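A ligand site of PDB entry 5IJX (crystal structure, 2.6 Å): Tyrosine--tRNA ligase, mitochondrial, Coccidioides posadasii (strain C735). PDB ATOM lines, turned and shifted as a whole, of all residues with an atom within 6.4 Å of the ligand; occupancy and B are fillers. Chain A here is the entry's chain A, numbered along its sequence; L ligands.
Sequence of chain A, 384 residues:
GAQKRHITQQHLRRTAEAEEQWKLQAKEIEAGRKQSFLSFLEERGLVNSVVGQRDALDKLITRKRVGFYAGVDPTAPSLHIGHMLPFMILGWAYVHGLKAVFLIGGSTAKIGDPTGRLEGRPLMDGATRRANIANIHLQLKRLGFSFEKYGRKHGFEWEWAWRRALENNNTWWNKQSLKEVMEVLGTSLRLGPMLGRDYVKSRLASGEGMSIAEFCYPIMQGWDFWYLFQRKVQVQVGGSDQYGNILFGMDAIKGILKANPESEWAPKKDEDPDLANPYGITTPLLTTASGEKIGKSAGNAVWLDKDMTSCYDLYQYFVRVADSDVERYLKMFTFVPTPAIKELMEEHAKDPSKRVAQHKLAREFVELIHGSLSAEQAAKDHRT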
ATOM      1  N   TYR A  69      24.647 -10.066  13.454  1.00  0.00           N
ATOM      2  CA  TYR A  69      24.289 -10.324  14.848  1.00  0.00           C
ATOM      3  C   TYR A  69      23.056 -11.209  14.917  1.00  0.00           C
ATOM      4  O   TYR A  69      22.180 -11.159  14.038  1.00  0.00           O
ATOM      5  CB  TYR A  69      24.080  -9.021  15.628  1.00  0.00           C
ATOM      6  CG  TYR A  69      22.639  -8.574  15.810  1.00  0.00           C
ATOM      7  CD1 TYR A  69      21.890  -8.998  16.902  1.00  0.00           C
ATOM      8  CD2 TYR A  69      22.035  -7.704  14.905  1.00  0.00           C
ATOM      9  CE1 TYR A  69      20.587  -8.591  17.072  1.00  0.00           C
ATOM     10  CE2 TYR A  69      20.732  -7.297  15.075  1.00  0.00           C
ATOM     11  CZ  TYR A  69      20.007  -7.741  16.159  1.00  0.00           C
ATOM     12  OH  TYR A  69      18.704  -7.334  16.329  1.00  0.00           O
ATOM     13  N   ALA A  70      23.008 -12.033  15.955  1.00  0.00           N
ATOM     14  CA  ALA A  70      21.868 -12.876  16.269  1.00  0.00           C
ATOM     15  C   ALA A  70      21.557 -12.746  17.747  1.00  0.00           C
ATOM     16  O   ALA A  70      22.462 -12.579  18.574  1.00  0.00           O
ATOM     17  CB  ALA A  70      22.124 -14.349  15.911  1.00  0.00           C
ATOM     18  N   GLY A  71      20.278 -12.810  18.078  1.00  0.00           N
ATOM     19  CA  GLY A  71      19.815 -12.604  19.447  1.00  0.00           C
ATOM     20  C   GLY A  71      19.110 -13.826  19.982  1.00  0.00           C
ATOM     21  O   GLY A  71      18.336 -14.469  19.269  1.00  0.00           O
ATOM     22  N   VAL A  72      19.369 -14.139  21.247  1.00  0.00           N
ATOM     23  CA  VAL A  72      18.689 -15.227  21.952  1.00  0.00           C
ATOM     24  C   VAL A  72      18.075 -14.663  23.221  1.00  0.00           C
ATOM     25  O   VAL A  72      18.743 -13.958  23.982  1.00  0.00           O
ATOM     26  CB  VAL A  72      19.644 -16.378  22.283  1.00  0.00           C
ATOM     27  CG1 VAL A  72      18.908 -17.471  23.043  1.00  0.00           C
ATOM     28  CG2 VAL A  72      20.250 -16.937  21.024  1.00  0.00           C
ATOM     29  N   ASP A  73      16.805 -14.965  23.437  1.00  0.00           N
ATOM     30  CA  ASP A  73      16.135 -14.572  24.671  1.00  0.00           C
ATOM     31  C   ASP A  73      16.383 -15.633  25.736  1.00  0.00           C
ATOM     32  O   ASP A  73      16.000 -16.792  25.530  1.00  0.00           O
ATOM     33  CB  ASP A  73      14.647 -14.391  24.445  1.00  0.00           C
ATOM     34  CG  ASP A  73      14.251 -12.925  24.329  1.00  0.00           C
ATOM     35  OD1 ASP A  73      15.142 -12.080  24.113  1.00  0.00           O
ATOM     36  OD2 ASP A  73      13.045 -12.632  24.462  1.00  0.00           O
ATOM     37  N   THR A  75      15.144 -17.524  27.805  1.00  0.00           N
ATOM     38  CA  THR A  75      13.957 -18.179  28.349  1.00  0.00           C
ATOM     39  C   THR A  75      14.150 -19.681  28.453  1.00  0.00           C
ATOM     40  O   THR A  75      13.189 -20.455  28.432  1.00  0.00           O
ATOM     41  CB  THR A  75      12.733 -17.848  27.497  1.00  0.00           C
ATOM     42  OG1 THR A  75      12.915 -18.366  26.167  1.00  0.00           O
ATOM     43  CG2 THR A  75      12.519 -16.351  27.429  1.00  0.00           C
ATOM     44  N   HIS A  83      19.262 -23.329  18.582  1.00  0.00           N
ATOM     45  CA  HIS A  83      19.818 -21.986  18.427  1.00  0.00           C
ATOM     46  C   HIS A  83      21.044 -21.945  17.513  1.00  0.00           C
ATOM     47  O   HIS A  83      21.498 -20.842  17.180  1.00  0.00           O
ATOM     48  CB  HIS A  83      20.220 -21.403  19.778  1.00  0.00           C
ATOM     49  CG  HIS A  83      19.092 -21.300  20.758  1.00  0.00           C
ATOM     50  ND1 HIS A  83      18.077 -20.375  20.636  1.00  0.00           N
ATOM     51  CD2 HIS A  83      18.836 -21.987  21.897  1.00  0.00           C
ATOM     52  CE1 HIS A  83      17.237 -20.504  21.653  1.00  0.00           C
ATOM     53  NE2 HIS A  83      17.675 -21.475  22.431  1.00  0.00           N
ATOM     54  N   LEU A 103      24.125 -11.623  20.762  1.00  0.00           N
ATOM     55  CA  LEU A 103      23.332 -10.755  21.629  1.00  0.00           C
ATOM     56  C   LEU A 103      22.430 -11.591  22.521  1.00  0.00           C
ATOM     57  O   LEU A 103      21.699 -12.466  22.038  1.00  0.00           O
ATOM     58  CB  LEU A 103      22.496  -9.770  20.816  1.00  0.00           C
ATOM     59  CG  LEU A 103      21.573  -8.848  21.634  1.00  0.00           C
ATOM     60  CD1 LEU A 103      22.377  -8.072  22.672  1.00  0.00           C
ATOM     61  CD2 LEU A 103      20.829  -7.901  20.720  1.00  0.00           C
ATOM     62  N   ILE A 104      22.479 -11.325  23.830  1.00  0.00           N
ATOM     63  CA  ILE A 104      21.584 -11.921  24.810  1.00  0.00           C
ATOM     64  C   ILE A 104      20.456 -10.935  25.070  1.00  0.00           C
ATOM     65  O   ILE A 104      20.693  -9.739  25.284  1.00  0.00           O
ATOM     66  CB  ILE A 104      22.322 -12.261  26.107  1.00  0.00           C
ATOM     67  CG1 ILE A 104      23.386 -13.338  25.851  1.00  0.00           C
ATOM     68  CG2 ILE A 104      21.357 -12.715  27.182  1.00  0.00           C
ATOM     69  N   GLY A 105      19.212 -11.427  25.070  1.00  0.00           N
ATOM     70  CA  GLY A 105      18.059 -10.571  25.278  1.00  0.00           C
ATOM     71  C   GLY A 105      17.720 -10.373  26.735  1.00  0.00           C
ATOM     72  O   GLY A 105      16.673 -10.840  27.208  1.00  0.00           O
ATOM     73  N   THR A 108      14.495  -7.945  26.673  1.00  0.00           N
ATOM     74  CA  THR A 108      13.426  -8.509  25.858  1.00  0.00           C
ATOM     75  C   THR A 108      12.856  -9.788  26.477  1.00  0.00           C
ATOM     76  O   THR A 108      11.665 -10.068  26.329  1.00  0.00           O
ATOM     77  CB  THR A 108      13.934  -8.786  24.445  1.00  0.00           C
ATOM     78  OG1 THR A 108      15.200  -9.457  24.514  1.00  0.00           O
ATOM     79  CG2 THR A 108      14.102  -7.487  23.676  1.00  0.00           C
ATOM     80  N   ASP A 113       9.102 -12.947  23.593  1.00  0.00           N
ATOM     81  CA  ASP A 113       8.766 -12.700  22.196  1.00  0.00           C
ATOM     82  C   ASP A 113       7.393 -13.301  21.895  1.00  0.00           C
ATOM     83  O   ASP A 113       7.227 -14.516  22.021  1.00  0.00           O
ATOM     84  CB  ASP A 113       9.820 -13.298  21.287  1.00  0.00           C
ATOM     85  CG  ASP A 113       9.679 -12.827  19.847  1.00  0.00           C
ATOM     86  OD1 ASP A 113       8.670 -12.153  19.544  1.00  0.00           O
ATOM     87  OD2 ASP A 113      10.570 -13.137  19.026  1.00  0.00           O
ATOM     88  N   THR A 115       6.002 -14.044  19.203  1.00  0.00           N
ATOM     89  CA  THR A 115       5.954 -14.942  18.060  1.00  0.00           C
ATOM     90  C   THR A 115       6.504 -16.309  18.485  1.00  0.00           C
ATOM     91  O   THR A 115       7.543 -16.351  19.136  1.00  0.00           O
ATOM     92  CB  THR A 115       6.758 -14.412  16.849  1.00  0.00           C
ATOM     93  OG1 THR A 115       6.603 -15.303  15.731  1.00  0.00           O
ATOM     94  CG2 THR A 115       8.229 -14.298  17.162  1.00  0.00           C
ATOM     95  N   ASN A 169      21.456  -6.802  25.605  1.00  0.00           N
ATOM     96  CA  ASN A 169      20.784  -5.598  25.165  1.00  0.00           C
ATOM     97  C   ASN A 169      20.415  -4.682  26.325  1.00  0.00           C
ATOM     98  O   ASN A 169      20.302  -3.463  26.121  1.00  0.00           O
ATOM     99  CB  ASN A 169      19.526  -5.940  24.342  1.00  0.00           C
ATOM    100  CG  ASN A 169      18.521  -6.764  25.111  1.00  0.00           C
ATOM    101  OD1 ASN A 169      18.640  -6.936  26.323  1.00  0.00           O
ATOM    102  ND2 ASN A 169      17.531  -7.280  24.398  1.00  0.00           N
ATOM    103  N   TYR A 217       7.144  -5.486  21.800  1.00  0.00           N
ATOM    104  CA  TYR A 217       8.340  -6.303  21.698  1.00  0.00           C
ATOM    105  C   TYR A 217       9.073  -6.089  20.374  1.00  0.00           C
ATOM    106  O   TYR A 217      10.287  -5.798  20.397  1.00  0.00           O
ATOM    107  CB  TYR A 217       7.980  -7.778  21.889  1.00  0.00           C
ATOM    108  CG  TYR A 217       9.170  -8.697  21.906  1.00  0.00           C
ATOM    109  CD1 TYR A 217       9.737  -9.111  23.107  1.00  0.00           C
ATOM    110  CD2 TYR A 217       9.742  -9.151  20.732  1.00  0.00           C
ATOM    111  CE1 TYR A 217      10.825  -9.949  23.133  1.00  0.00           C
ATOM    112  CE2 TYR A 217      10.842  -9.991  20.740  1.00  0.00           C
ATOM    113  CZ  TYR A 217      11.375 -10.389  21.943  1.00  0.00           C
ATOM    114  OH  TYR A 217      12.470 -11.220  21.953  1.00  0.00           O
ATOM    115  N   MET A 220      11.176  -3.018  20.478  1.00  0.00           N
ATOM    116  CA  MET A 220      12.403  -3.118  21.250  1.00  0.00           C
ATOM    117  C   MET A 220      13.466  -3.854  20.442  1.00  0.00           C
ATOM    118  O   MET A 220      14.619  -3.435  20.395  1.00  0.00           O
ATOM    119  CB  MET A 220      12.166  -3.847  22.568  1.00  0.00           C
ATOM    120  CG  MET A 220      11.250  -3.102  23.516  1.00  0.00           C
ATOM    121  SD  MET A 220      11.171  -3.989  25.251  1.00  0.00           S
ATOM    122  CE  MET A 220      12.756  -3.223  26.065  1.00  0.00           C
ATOM    123  N   GLN A 221      13.062  -4.950  19.783  1.00  0.00           N
ATOM    124  CA  GLN A 221      14.024  -5.707  18.991  1.00  0.00           C
ATOM    125  C   GLN A 221      14.521  -4.875  17.809  1.00  0.00           C
ATOM    126  O   GLN A 221      15.726  -4.877  17.500  1.00  0.00           O
ATOM    127  CB  GLN A 221      13.399  -7.008  18.525  1.00  0.00           C
ATOM    128  CG  GLN A 221      14.265  -7.800  17.570  1.00  0.00           C
ATOM    129  CD  GLN A 221      13.854  -9.254  17.466  1.00  0.00           C
ATOM    130  OE1 GLN A 221      13.058  -9.735  18.269  1.00  0.00           O
ATOM    131  NE2 GLN A 221      14.387  -9.953  16.480  1.00  0.00           N
ATOM    132  N   GLY A 222      13.619  -4.155  17.141  1.00  0.00           N
ATOM    133  CA  GLY A 222      14.046  -3.254  16.083  1.00  0.00           C
ATOM    134  C   GLY A 222      15.004  -2.195  16.580  1.00  0.00           C
ATOM    135  O   GLY A 222      15.902  -1.772  15.835  1.00  0.00           O
ATOM    136  N   ASP A 224      17.125  -2.616  19.169  1.00  0.00           N
ATOM    137  CA  ASP A 224      18.400  -3.317  19.242  1.00  0.00           C
ATOM    138  C   ASP A 224      19.096  -3.301  17.892  1.00  0.00           C
ATOM    139  O   ASP A 224      20.286  -2.967  17.782  1.00  0.00           O
ATOM    140  CB  ASP A 224      18.187  -4.763  19.722  1.00  0.00           C
ATOM    141  CG  ASP A 224      17.725  -4.852  21.149  1.00  0.00           C
ATOM    142  OD1 ASP A 224      17.778  -3.826  21.877  1.00  0.00           O
ATOM    143  OD2 ASP A 224      17.316  -5.958  21.571  1.00  0.00           O
ATOM    144  N   PHE A 225      18.344  -3.635  16.833  1.00  0.00           N
ATOM    145  CA  PHE A 225      18.912  -3.617  15.485  1.00  0.00           C
ATOM    146  C   PHE A 225      19.432  -2.234  15.118  1.00  0.00           C
ATOM    147  O   PHE A 225      20.491  -2.114  14.500  1.00  0.00           O
ATOM    148  CB  PHE A 225      17.856  -4.073  14.474  1.00  0.00           C
ATOM    149  CG  PHE A 225      18.421  -4.493  13.146  1.00  0.00           C
ATOM    150  CD1 PHE A 225      19.781  -4.396  12.865  1.00  0.00           C
ATOM    151  CD2 PHE A 225      17.585  -4.997  12.157  1.00  0.00           C
ATOM    152  CE1 PHE A 225      20.287  -4.787  11.652  1.00  0.00           C
ATOM    153  CE2 PHE A 225      18.092  -5.396  10.928  1.00  0.00           C
ATOM    154  CZ  PHE A 225      19.439  -5.289  10.681  1.00  0.00           C
ATOM    155  N   LEU A 228      22.736  -1.456  17.100  1.00  0.00           N
ATOM    156  CA  LEU A 228      23.873  -2.116  16.484  1.00  0.00           C
ATOM    157  C   LEU A 228      24.135  -1.610  15.076  1.00  0.00           C
ATOM    158  O   LEU A 228      25.266  -1.679  14.590  1.00  0.00           O
ATOM    159  CB  LEU A 228      23.638  -3.628  16.460  1.00  0.00           C
ATOM    160  CG  LEU A 228      23.495  -4.271  17.832  1.00  0.00           C
ATOM    161  CD1 LEU A 228      23.109  -5.732  17.713  1.00  0.00           C
ATOM    162  CD2 LEU A 228      24.784  -4.114  18.630  1.00  0.00           C
ATOM    163  N   GLN A 236      21.007  -8.789  10.253  1.00  0.00           N
ATOM    164  CA  GLN A 236      20.481  -9.537  11.385  1.00  0.00           C
ATOM    165  C   GLN A 236      20.161 -10.956  10.951  1.00  0.00           C
ATOM    166  O   GLN A 236      19.500 -11.168   9.925  1.00  0.00           O
ATOM    167  CB  GLN A 236      19.226  -8.889  11.978  1.00  0.00           C
ATOM    168  CG  GLN A 236      18.780  -9.545  13.301  1.00  0.00           C
ATOM    169  CD  GLN A 236      17.528  -8.946  13.922  1.00  0.00           C
ATOM    170  OE1 GLN A 236      16.968  -9.531  14.860  1.00  0.00           O
ATOM    171  NE2 GLN A 236      17.093  -7.803  13.425  1.00  0.00           N
ATOM    172  N   ASP A 241      11.382 -18.528  12.144  1.00  0.00           N
ATOM    173  CA  ASP A 241      10.284 -17.889  12.874  1.00  0.00           C
ATOM    174  C   ASP A 241      10.516 -16.393  13.054  1.00  0.00           C
ATOM    175  O   ASP A 241       9.552 -15.630  13.182  1.00  0.00           O
ATOM    176  CB  ASP A 241      10.129 -18.560  14.241  1.00  0.00           C
ATOM    177  CG  ASP A 241      11.361 -18.399  15.108  1.00  0.00           C
ATOM    178  OD1 ASP A 241      12.399 -19.027  14.811  1.00  0.00           O
ATOM    179  OD2 ASP A 241      11.299 -17.636  16.099  1.00  0.00           O
ATOM    180  N   GLN A 242      11.775 -15.952  13.064  1.00  0.00           N
ATOM    181  CA  GLN A 242      12.087 -14.565  13.330  1.00  0.00           C
ATOM    182  C   GLN A 242      11.976 -13.680  12.104  1.00  0.00           C
ATOM    183  O   GLN A 242      12.208 -12.470  12.217  1.00  0.00           O
ATOM    184  CB  GLN A 242      13.493 -14.460  13.915  1.00  0.00           C
ATOM    185  CG  GLN A 242      13.602 -15.003  15.335  1.00  0.00           C
ATOM    186  CD  GLN A 242      12.878 -14.122  16.344  1.00  0.00           C
ATOM    187  OE1 GLN A 242      13.233 -12.963  16.537  1.00  0.00           O
ATOM    188  NE2 GLN A 242      11.862 -14.681  16.991  1.00  0.00           N
ATOM    189  N   ASN A 245      10.114 -10.465  12.636  1.00  0.00           N
ATOM    190  CA  ASN A 245      10.821  -9.516  13.489  1.00  0.00           C
ATOM    191  C   ASN A 245      11.980  -8.867  12.754  1.00  0.00           C
ATOM    192  O   ASN A 245      12.305  -7.700  13.008  1.00  0.00           O
ATOM    193  CB  ASN A 245      11.327 -10.213  14.758  1.00  0.00           C
ATOM    194  CG  ASN A 245      10.213 -10.502  15.740  1.00  0.00           C
ATOM    195  OD1 ASN A 245       9.096  -9.992  15.602  1.00  0.00           O
ATOM    196  ND2 ASN A 245      10.501 -11.326  16.742  1.00  0.00           N
HETATM  197  N1  LIG L   1      13.431 -12.884  19.323  1.00  0.00           N
HETATM  198  C1  LIG L   1      14.527 -13.780  19.657  1.00  0.00           C
HETATM  199  C2  LIG L   1      14.004 -15.103  20.210  1.00  0.00           C
HETATM  200  O1  LIG L   1      14.658 -16.151  20.131  1.00  0.00           O
HETATM  201  C3  LIG L   1      15.460 -13.117  20.684  1.00  0.00           C
HETATM  202  C4  LIG L   1      15.998 -11.763  20.268  1.00  0.00           C
HETATM  203  C5  LIG L   1      16.331 -11.496  18.948  1.00  0.00           C
HETATM  204  C6  LIG L   1      16.170 -10.752  21.196  1.00  0.00           C
HETATM  205  C7  LIG L   1      16.823 -10.263  18.567  1.00  0.00           C
HETATM  206  C8  LIG L   1      16.662  -9.510  20.830  1.00  0.00           C
HETATM  207  C9  LIG L   1      16.992  -9.268  19.511  1.00  0.00           C
HETATM  208  O2  LIG L   1      17.480  -8.030  19.153  1.00  0.00           O
HETATM  209  O3  LIG L   1      12.893 -15.171  20.755  1.00  0.00           O
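N1 of the ligand lies within hydrogen-bond range of OE1 of Gln 242 (2.8 Å). The side-chain carboxylate (OD2) of Asp 113 is in salt-bridge range of a nitrogen (N1) of the ligand, at 2.9 Å. OH of Tyr 69 is in hydrogen-bond range of O2 of the ligand, at 3.2 Å. OD2 of Asp 224 is in hydrogen-bond range of O2 of the ligand (3.2 Å). A nitrogen (N1) of the ligand lies within hydrogen-bond range of the side-chain amide oxygen (OE1) of Gln 221 (3.3 Å). The side-chain hydroxyl (OH) of Tyr 217 lies within hydrogen-bond range of a nitrogen (N1) of the ligand, 3.3 Å away.
The side-chain amide oxygen (OE1) of Gln 242 sits at hydrogen-bond distance from the side-chain amide nitrogen (NE2) of Gln 221, at 3.2 Å. The side-chain amide oxygen (OE1) of Gln 242 lies within hydrogen-bond range of the side-chain amide nitrogen (ND2) of Asn 245, 3.2 Å away. The side-chain carboxylate of Asp 113 is in hydrogen-bond range of the side-chain amide nitrogen of Asn 245 (2.9 Å). The side-chain carboxylate of Asp 113 sits close to the backbone NH of Thr 115, 3.3 Å away. The side-chain carboxylate (OD2) of Asp 224 is in hydrogen-bond range of the side-chain amide nitrogen (ND2) of Asn 169 (3.1 Å). N of Val 72 sits at hydrogen-bond distance from O of Leu 103 (3.0 Å). O of Ala 70 lies within hydrogen-bond range of N of Leu 103, 2.9 Å away. N of Gly 105 lies within hydrogen-bond range of O of Val 72 (2.8 Å).
Residues that only touch the ligand: Asp 73 (3.4 Å), Gly 71 (3.5 Å), Thr 108 (3.7 Å), Leu 103 (3.7 Å), Gln 236 (3.8 Å) and Val 72 (3.96 Å).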
